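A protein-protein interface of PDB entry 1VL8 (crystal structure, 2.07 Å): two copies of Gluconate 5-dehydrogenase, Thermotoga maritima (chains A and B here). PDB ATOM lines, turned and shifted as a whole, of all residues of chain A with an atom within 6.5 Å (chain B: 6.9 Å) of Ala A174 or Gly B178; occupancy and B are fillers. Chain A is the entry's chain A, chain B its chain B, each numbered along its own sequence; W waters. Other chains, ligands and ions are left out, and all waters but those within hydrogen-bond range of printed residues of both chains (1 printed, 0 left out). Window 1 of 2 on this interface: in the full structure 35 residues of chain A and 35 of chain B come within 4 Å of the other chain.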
ATOM      1  N   PHE A 123       6.469  -6.764  30.498  1.00  0.00           N
ATOM      2  CA  PHE A 123       6.954  -6.578  29.145  1.00  0.00           C
ATOM      3  C   PHE A 123       8.058  -5.509  29.136  1.00  0.00           C
ATOM      4  O   PHE A 123       9.125  -5.708  28.576  1.00  0.00           O
ATOM      5  CB  PHE A 123       5.823  -6.171  28.176  1.00  0.00           C
ATOM      6  CG  PHE A 123       6.225  -6.208  26.731  1.00  0.00           C
ATOM      7  CD1 PHE A 123       6.867  -5.131  26.147  1.00  0.00           C
ATOM      8  CD2 PHE A 123       5.957  -7.329  25.943  1.00  0.00           C
ATOM      9  CE1 PHE A 123       7.251  -5.175  24.805  1.00  0.00           C
ATOM     10  CE2 PHE A 123       6.335  -7.380  24.612  1.00  0.00           C
ATOM     11  CZ  PHE A 123       6.980  -6.295  24.033  1.00  0.00           C
ATOM     12  N   ILE A 127      12.692  -5.529  28.750  1.00  0.00           N
ATOM     13  CA  ILE A 127      13.416  -4.630  27.843  1.00  0.00           C
ATOM     14  C   ILE A 127      14.288  -3.646  28.638  1.00  0.00           C
ATOM     15  O   ILE A 127      15.405  -3.336  28.270  1.00  0.00           O
ATOM     16  CB  ILE A 127      12.417  -3.945  26.934  1.00  0.00           C
ATOM     17  CG1 ILE A 127      11.949  -4.959  25.839  1.00  0.00           C
ATOM     18  CG2 ILE A 127      12.987  -2.637  26.352  1.00  0.00           C
ATOM     19  CD1 ILE A 127      10.603  -4.792  25.401  1.00  0.00           C
ATOM     20  N   LEU A 131      17.878  -4.565  27.329  1.00  0.00           N
ATOM     21  CA  LEU A 131      18.208  -3.631  26.282  1.00  0.00           C
ATOM     22  C   LEU A 131      18.636  -2.277  26.867  1.00  0.00           C
ATOM     23  O   LEU A 131      19.727  -1.852  26.617  1.00  0.00           O
ATOM     24  CB  LEU A 131      17.013  -3.455  25.334  1.00  0.00           C
ATOM     25  CG  LEU A 131      17.112  -2.409  24.237  1.00  0.00           C
ATOM     26  CD1 LEU A 131      18.315  -2.771  23.358  1.00  0.00           C
ATOM     27  CD2 LEU A 131      15.806  -2.245  23.439  1.00  0.00           C
ATOM     28  N   THR A 160      16.756 -15.417  19.248  1.00  0.00           N
ATOM     29  CA  THR A 160      15.660 -14.456  18.975  1.00  0.00           C
ATOM     30  C   THR A 160      16.083 -13.177  18.214  1.00  0.00           C
ATOM     31  O   THR A 160      15.248 -12.446  17.676  1.00  0.00           O
ATOM     32  CB  THR A 160      14.886 -14.043  20.270  1.00  0.00           C
ATOM     33  OG1 THR A 160      15.738 -13.318  21.195  1.00  0.00           O
ATOM     34  CG2 THR A 160      14.294 -15.248  20.932  1.00  0.00           C
ATOM     35  N   ILE A 169       7.610 -15.619  24.612  1.00  0.00           N
ATOM     36  CA  ILE A 169       8.792 -14.854  24.907  1.00  0.00           C
ATOM     37  C   ILE A 169       8.905 -13.574  24.048  1.00  0.00           C
ATOM     38  O   ILE A 169      10.009 -13.190  23.672  1.00  0.00           O
ATOM     39  CB  ILE A 169      10.079 -15.727  24.788  1.00  0.00           C
ATOM     40  CG1 ILE A 169      10.182 -16.358  23.385  1.00  0.00           C
ATOM     41  CG2 ILE A 169      10.128 -16.794  25.905  1.00  0.00           C
ATOM     42  CD1 ILE A 169      11.547 -16.877  23.072  1.00  0.00           C
ATOM     43  N   SER A 170       7.775 -12.930  23.735  1.00  0.00           N
ATOM     44  CA  SER A 170       7.765 -11.704  22.874  1.00  0.00           C
ATOM     45  C   SER A 170       8.619 -10.561  23.409  1.00  0.00           C
ATOM     46  O   SER A 170       9.391  -9.995  22.643  1.00  0.00           O
ATOM     47  CB  SER A 170       6.330 -11.189  22.623  1.00  0.00           C
ATOM     48  OG  SER A 170       5.665 -10.855  23.834  1.00  0.00           O
ATOM     49  N   ALA A 171       8.524 -10.272  24.731  1.00  0.00           N
ATOM     50  CA  ALA A 171       9.341  -9.191  25.318  1.00  0.00           C
ATOM     51  C   ALA A 171      10.832  -9.460  25.207  1.00  0.00           C
ATOM     52  O   ALA A 171      11.630  -8.598  24.803  1.00  0.00           O
ATOM     53  CB  ALA A 171       8.965  -8.931  26.785  1.00  0.00           C
ATOM     54  N   TYR A 172      11.202 -10.683  25.551  1.00  0.00           N
ATOM     55  CA  TYR A 172      12.586 -11.108  25.463  1.00  0.00           C
ATOM     56  C   TYR A 172      13.163 -11.017  24.035  1.00  0.00           C
ATOM     57  O   TYR A 172      14.248 -10.466  23.832  1.00  0.00           O
ATOM     58  CB  TYR A 172      12.653 -12.529  25.969  1.00  0.00           C
ATOM     59  CG  TYR A 172      14.013 -13.146  26.030  1.00  0.00           C
ATOM     60  CD1 TYR A 172      14.853 -12.880  27.092  1.00  0.00           C
ATOM     61  CD2 TYR A 172      14.446 -14.034  25.046  1.00  0.00           C
ATOM     62  CE1 TYR A 172      16.077 -13.486  27.207  1.00  0.00           C
ATOM     63  CE2 TYR A 172      15.689 -14.636  25.132  1.00  0.00           C
ATOM     64  CZ  TYR A 172      16.506 -14.353  26.210  1.00  0.00           C
ATOM     65  OH  TYR A 172      17.718 -14.945  26.346  1.00  0.00           O
ATOM     66  N   ALA A 173      12.402 -11.551  23.074  1.00  0.00           N
ATOM     67  CA  ALA A 173      12.766 -11.482  21.670  1.00  0.00           C
ATOM     68  C   ALA A 173      12.998 -10.045  21.257  1.00  0.00           C
ATOM     69  O   ALA A 173      13.990  -9.801  20.600  1.00  0.00           O
ATOM     70  CB  ALA A 173      11.709 -12.120  20.817  1.00  0.00           C
ATOM     71  N   ALA A 174      12.047  -9.133  21.596  1.00  0.00           N
ATOM     72  CA  ALA A 174      12.153  -7.732  21.237  1.00  0.00           C
ATOM     73  C   ALA A 174      13.446  -7.118  21.825  1.00  0.00           C
ATOM     74  O   ALA A 174      14.158  -6.381  21.158  1.00  0.00           O
ATOM     75  CB  ALA A 174      10.932  -6.970  21.698  1.00  0.00           C
ATOM     76  N   SER A 175      13.728  -7.447  23.087  1.00  0.00           N
ATOM     77  CA  SER A 175      14.932  -6.974  23.762  1.00  0.00           C
ATOM     78  C   SER A 175      16.222  -7.372  23.016  1.00  0.00           C
ATOM     79  O   SER A 175      17.165  -6.565  22.910  1.00  0.00           O
ATOM     80  CB  SER A 175      14.949  -7.425  25.256  1.00  0.00           C
ATOM     81  OG  SER A 175      15.450  -8.768  25.414  1.00  0.00           O
ATOM     82  N   LYS A 176      16.277  -8.629  22.560  1.00  0.00           N
ATOM     83  CA  LYS A 176      17.479  -9.186  21.970  1.00  0.00           C
ATOM     84  C   LYS A 176      17.671  -8.703  20.531  1.00  0.00           C
ATOM     85  O   LYS A 176      18.780  -8.471  20.154  1.00  0.00           O
ATOM     86  CB  LYS A 176      17.489 -10.719  22.051  1.00  0.00           C
ATOM     87  CG  LYS A 176      17.426 -11.243  23.496  1.00  0.00           C
ATOM     88  CD  LYS A 176      18.720 -10.923  24.210  1.00  0.00           C
ATOM     89  CE  LYS A 176      18.865 -11.576  25.556  1.00  0.00           C
ATOM     90  NZ  LYS A 176      20.144 -11.169  26.213  1.00  0.00           N
ATOM     91  N   GLY A 177      16.595  -8.545  19.752  1.00  0.00           N
ATOM     92  CA  GLY A 177      16.694  -7.861  18.455  1.00  0.00           C
ATOM     93  C   GLY A 177      17.106  -6.400  18.630  1.00  0.00           C
ATOM     94  O   GLY A 177      17.804  -5.823  17.801  1.00  0.00           O
ATOM     95  N   GLY A 178      16.637  -5.785  19.705  1.00  0.00           N
ATOM     96  CA  GLY A 178      17.069  -4.474  20.070  1.00  0.00           C
ATOM     97  C   GLY A 178      18.552  -4.398  20.343  1.00  0.00           C
ATOM     98  O   GLY A 178      19.242  -3.480  19.887  1.00  0.00           O
ATOM     99  N   VAL A 179      19.031  -5.370  21.117  1.00  0.00           N
ATOM    100  CA  VAL A 179      20.461  -5.476  21.404  1.00  0.00           C
ATOM    101  C   VAL A 179      21.313  -5.622  20.118  1.00  0.00           C
ATOM    102  O   VAL A 179      22.360  -4.969  20.020  1.00  0.00           O
ATOM    103  CB  VAL A 179      20.767  -6.622  22.417  1.00  0.00           C
ATOM    104  CG1 VAL A 179      22.275  -6.986  22.404  1.00  0.00           C
ATOM    105  CG2 VAL A 179      20.240  -6.311  23.801  1.00  0.00           C
ATOM    106  N   SER A 181      20.633  -4.603  17.003  1.00  0.00           N
ATOM    107  CA  SER A 181      20.690  -3.361  16.271  1.00  0.00           C
ATOM    108  C   SER A 181      21.461  -2.264  17.002  1.00  0.00           C
ATOM    109  O   SER A 181      22.184  -1.533  16.357  1.00  0.00           O
ATOM    110  CB  SER A 181      19.334  -2.865  15.945  1.00  0.00           C
ATOM    111  OG  SER A 181      18.819  -3.578  14.859  1.00  0.00           O
ATOM    112  N   LEU B 131       8.698   0.875  19.764  1.00  0.00           N
ATOM    113  CA  LEU B 131       8.710  -0.536  20.098  1.00  0.00           C
ATOM    114  C   LEU B 131       7.576  -0.872  21.047  1.00  0.00           C
ATOM    115  O   LEU B 131       6.728  -1.689  20.701  1.00  0.00           O
ATOM    116  CB  LEU B 131      10.052  -0.950  20.712  1.00  0.00           C
ATOM    117  CG  LEU B 131      10.168  -2.393  21.213  1.00  0.00           C
ATOM    118  CD1 LEU B 131       9.780  -3.437  20.085  1.00  0.00           C
ATOM    119  CD2 LEU B 131      11.588  -2.677  21.785  1.00  0.00           C
ATOM    120  N   VAL B 161      17.211  -2.424  11.151  1.00  0.00           N
ATOM    121  CA  VAL B 161      17.001  -3.814  11.420  1.00  0.00           C
ATOM    122  C   VAL B 161      18.237  -4.633  11.006  1.00  0.00           C
ATOM    123  O   VAL B 161      18.552  -5.623  11.631  1.00  0.00           O
ATOM    124  CB  VAL B 161      15.723  -4.337  10.677  1.00  0.00           C
ATOM    125  CG1 VAL B 161      15.666  -5.835  10.707  1.00  0.00           C
ATOM    126  CG2 VAL B 161      14.473  -3.672  11.303  1.00  0.00           C
ATOM    127  N   TYR B 172      16.881   4.668  18.052  1.00  0.00           N
ATOM    128  CA  TYR B 172      16.043   4.313  16.929  1.00  0.00           C
ATOM    129  C   TYR B 172      16.401   2.942  16.372  1.00  0.00           C
ATOM    130  O   TYR B 172      15.539   2.103  16.164  1.00  0.00           O
ATOM    131  CB  TYR B 172      16.236   5.385  15.849  1.00  0.00           C
ATOM    132  CG  TYR B 172      15.383   5.225  14.626  1.00  0.00           C
ATOM    133  CD1 TYR B 172      14.044   5.614  14.626  1.00  0.00           C
ATOM    134  CD2 TYR B 172      15.920   4.741  13.441  1.00  0.00           C
ATOM    135  CE1 TYR B 172      13.264   5.530  13.460  1.00  0.00           C
ATOM    136  CE2 TYR B 172      15.157   4.628  12.287  1.00  0.00           C
ATOM    137  CZ  TYR B 172      13.825   5.039  12.292  1.00  0.00           C
ATOM    138  OH  TYR B 172      13.062   4.927  11.158  1.00  0.00           O
ATOM    139  N   ALA B 173      17.676   2.735  16.107  1.00  0.00           N
ATOM    140  CA  ALA B 173      18.162   1.410  15.668  1.00  0.00           C
ATOM    141  C   ALA B 173      17.692   0.295  16.619  1.00  0.00           C
ATOM    142  O   ALA B 173      17.185  -0.726  16.179  1.00  0.00           O
ATOM    143  CB  ALA B 173      19.716   1.416  15.571  1.00  0.00           C
ATOM    144  N   ALA B 174      17.912   0.502  17.915  1.00  0.00           N
ATOM    145  CA  ALA B 174      17.471  -0.442  18.925  1.00  0.00           C
ATOM    146  C   ALA B 174      15.992  -0.735  18.810  1.00  0.00           C
ATOM    147  O   ALA B 174      15.587  -1.897  18.841  1.00  0.00           O
ATOM    148  CB  ALA B 174      17.857   0.052  20.329  1.00  0.00           C
ATOM    149  N   SER B 175      15.180   0.313  18.698  1.00  0.00           N
ATOM    150  CA  SER B 175      13.736   0.160  18.584  1.00  0.00           C
ATOM    151  C   SER B 175      13.313  -0.712  17.376  1.00  0.00           C
ATOM    152  O   SER B 175      12.415  -1.584  17.494  1.00  0.00           O
ATOM    153  CB  SER B 175      13.027   1.541  18.607  1.00  0.00           C
ATOM    154  OG  SER B 175      13.084   2.198  17.347  1.00  0.00           O
ATOM    155  N   LYS B 176      13.974  -0.497  16.240  1.00  0.00           N
ATOM    156  CA  LYS B 176      13.633  -1.156  14.996  1.00  0.00           C
ATOM    157  C   LYS B 176      14.105  -2.592  14.959  1.00  0.00           C
ATOM    158  O   LYS B 176      13.378  -3.431  14.485  1.00  0.00           O
ATOM    159  CB  LYS B 176      14.163  -0.379  13.786  1.00  0.00           C
ATOM    160  CG  LYS B 176      13.506   1.026  13.703  1.00  0.00           C
ATOM    161  CD  LYS B 176      11.983   0.964  13.459  1.00  0.00           C
ATOM    162  CE  LYS B 176      11.379   2.374  13.155  1.00  0.00           C
ATOM    163  NZ  LYS B 176       9.956   2.262  12.857  1.00  0.00           N
ATOM    164  N   GLY B 177      15.277  -2.866  15.500  1.00  0.00           N
ATOM    165  CA  GLY B 177      15.709  -4.252  15.695  1.00  0.00           C
ATOM    166  C   GLY B 177      14.760  -4.980  16.647  1.00  0.00           C
ATOM    167  O   GLY B 177      14.473  -6.170  16.475  1.00  0.00           O
ATOM    168  N   GLY B 178      14.283  -4.269  17.679  1.00  0.00           N
ATOM    169  CA  GLY B 178      13.280  -4.838  18.555  1.00  0.00           C
ATOM    170  C   GLY B 178      11.947  -5.156  17.861  1.00  0.00           C
ATOM    171  O   GLY B 178      11.310  -6.179  18.175  1.00  0.00           O
ATOM    172  N   VAL B 179      11.502  -4.252  16.982  1.00  0.00           N
ATOM    173  CA  VAL B 179      10.309  -4.459  16.192  1.00  0.00           C
ATOM    174  C   VAL B 179      10.434  -5.699  15.301  1.00  0.00           C
ATOM    175  O   VAL B 179       9.492  -6.477  15.224  1.00  0.00           O
ATOM    176  CB  VAL B 179       9.943  -3.237  15.341  1.00  0.00           C
ATOM    177  CG1 VAL B 179       8.906  -3.620  14.202  1.00  0.00           C
ATOM    178  CG2 VAL B 179       9.427  -2.130  16.214  1.00  0.00           C
ATOM    179  N   ALA B 180      11.587  -5.882  14.646  1.00  0.00           N
ATOM    180  CA  ALA B 180      11.821  -7.050  13.842  1.00  0.00           C
ATOM    181  C   ALA B 180      11.671  -8.349  14.633  1.00  0.00           C
ATOM    182  O   ALA B 180      11.023  -9.271  14.167  1.00  0.00           O
ATOM    183  CB  ALA B 180      13.227  -6.989  13.168  1.00  0.00           C
ATOM    184  N   SER B 181      12.350  -8.449  15.782  1.00  0.00           N
ATOM    185  CA  SER B 181      12.291  -9.667  16.586  1.00  0.00           C
ATOM    186  C   SER B 181      10.892  -9.867  17.221  1.00  0.00           C
ATOM    187  O   SER B 181      10.404 -11.019  17.305  1.00  0.00           O
ATOM    188  CB  SER B 181      13.400  -9.694  17.648  1.00  0.00           C
ATOM    189  OG  SER B 181      14.625 -10.025  17.025  1.00  0.00           O
ATOM    190  N   LEU B 182      10.269  -8.768  17.661  1.00  0.00           N
ATOM    191  CA  LEU B 182       8.876  -8.790  18.132  1.00  0.00           C
ATOM    192  C   LEU B 182       7.915  -9.375  17.067  1.00  0.00           C
ATOM    193  O   LEU B 182       7.088 -10.289  17.329  1.00  0.00           O
ATOM    194  CB  LEU B 182       8.421  -7.378  18.591  1.00  0.00           C
ATOM    195  CG  LEU B 182       6.914  -7.308  18.949  1.00  0.00           C
ATOM    196  CD1 LEU B 182       6.661  -8.122  20.219  1.00  0.00           C
ATOM    197  CD2 LEU B 182       6.446  -5.823  19.093  1.00  0.00           C
ATOM    198  N   THR B 183       8.110  -8.904  15.846  1.00  0.00           N
ATOM    199  CA  THR B 183       7.349  -9.345  14.694  1.00  0.00           C
ATOM    200  C   THR B 183       7.467 -10.855  14.501  1.00  0.00           C
ATOM    201  O   THR B 183       6.443 -11.542  14.367  1.00  0.00           O
ATOM    202  CB  THR B 183       7.769  -8.584  13.429  1.00  0.00           C
ATOM    203  OG1 THR B 183       7.460  -7.215  13.586  1.00  0.00           O
ATOM    204  CG2 THR B 183       7.082  -9.118  12.205  1.00  0.00           C
ATOM    205  N   LYS B 184       8.690 -11.368  14.624  1.00  0.00           N
ATOM    206  CA  LYS B 184       8.926 -12.805  14.556  1.00  0.00           C
ATOM    207  C   LYS B 184       8.229 -13.590  15.676  1.00  0.00           C
ATOM    208  O   LYS B 184       7.643 -14.615  15.407  1.00  0.00           O
ATOM    209  CB  LYS B 184      10.415 -13.112  14.500  1.00  0.00           C
ATOM    210  CG  LYS B 184      11.032 -12.612  13.218  1.00  0.00           C
ATOM    211  CD  LYS B 184      12.492 -12.701  13.223  1.00  0.00           C
ATOM    212  CE  LYS B 184      13.018 -12.319  11.800  1.00  0.00           C
ATOM    213  NZ  LYS B 184      14.445 -12.552  11.738  1.00  0.00           N
ATOM    214  N   ALA B 185       8.306 -13.088  16.913  1.00  0.00           N
ATOM    215  CA  ALA B 185       7.651 -13.690  18.043  1.00  0.00           C
ATOM    216  C   ALA B 185       6.146 -13.759  17.860  1.00  0.00           C
ATOM    217  O   ALA B 185       5.512 -14.807  18.148  1.00  0.00           O
ATOM    218  CB  ALA B 185       8.012 -12.947  19.335  1.00  0.00           C
HETATM  219  O   HOH W   1      18.326  -6.540  14.577  1.00  0.00           O
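Ala A173 touches Ser B181, and with the chains exchanged Ser A181 touches Ala B173. Ala A174 touches Gly B178, and with the chains exchanged Gly A178 touches Ala B174. Gly B177 touches its own counterpart, Gly A177. Gly A178 touches its own counterpart, Gly B178. Of the 14 pairs that touch across the chains among the printed residues, 10 have their exchanged pair printed and touching as well.
Of the printed residues of chain B, Thr A160 touches Ser B181 (2.6 Å). Ala A171 touches none of the printed residues of chain B. Of the printed residues of chain B, Ala A174 touches Gly B178. Printed residues of chain B within 4 Å of Gly A177: Gly B177 (3.4 Å), Gly B178 (3.7 Å) and Ser B181 (3.3 Å). Of the printed residues of chain A, Ala B173 touches Ser A181 (3.0 Å). Of the printed residues of chain A, Gly B178 touches Ala A174, Gly A177 and Gly A178.
Water W1 lies within hydrogen-bond range of the side-chain hydroxyl (OG) of Ser A181 (3.0 Å), the backbone carbonyl oxygen (O) of Val B161 (3.1 Å) and the backbone carbonyl oxygen (O) of Gly A177 (3.3 Å).
O of Thr A160 sits at hydrogen-bond distance from OG of Ser B181. N of Gly B178 sits close to N of Gly A178, 3.5 Å away.
Hydrophobic or aromatic side chains of chain A within 4 Å of the printed part of chain B: Ala A173 and Ala A174. Among the printed residues, no Asp or Glu carboxylate lies within 4 Å of a Lys or Arg side-chain nitrogen of the other chain.
Leu B182 touches Ser A170 (CD1 to CB, 3.9 Å). Ser B181 touches Ala A173 (CB to O, 3.0 Å). Ala A174 touches Gly B178 (O to CA, 3.2 Å). CA of Gly B177 touches O of Gly A177, 3.4 Å away. Gly A177 touches Gly B178. Gly A177 touches Ser B181 (CA to OG, 3.3 Å). Ala B174 touches Gly A178 (O to CA, 3.2 Å). C of Gly B177 touches N of Gly A178, 3.7 Å away. CB of Ser A181 touches O of Ala B173, 3.0 Å away. OG of Ser A181 touches CA of Gly B177, 3.3 Å away.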
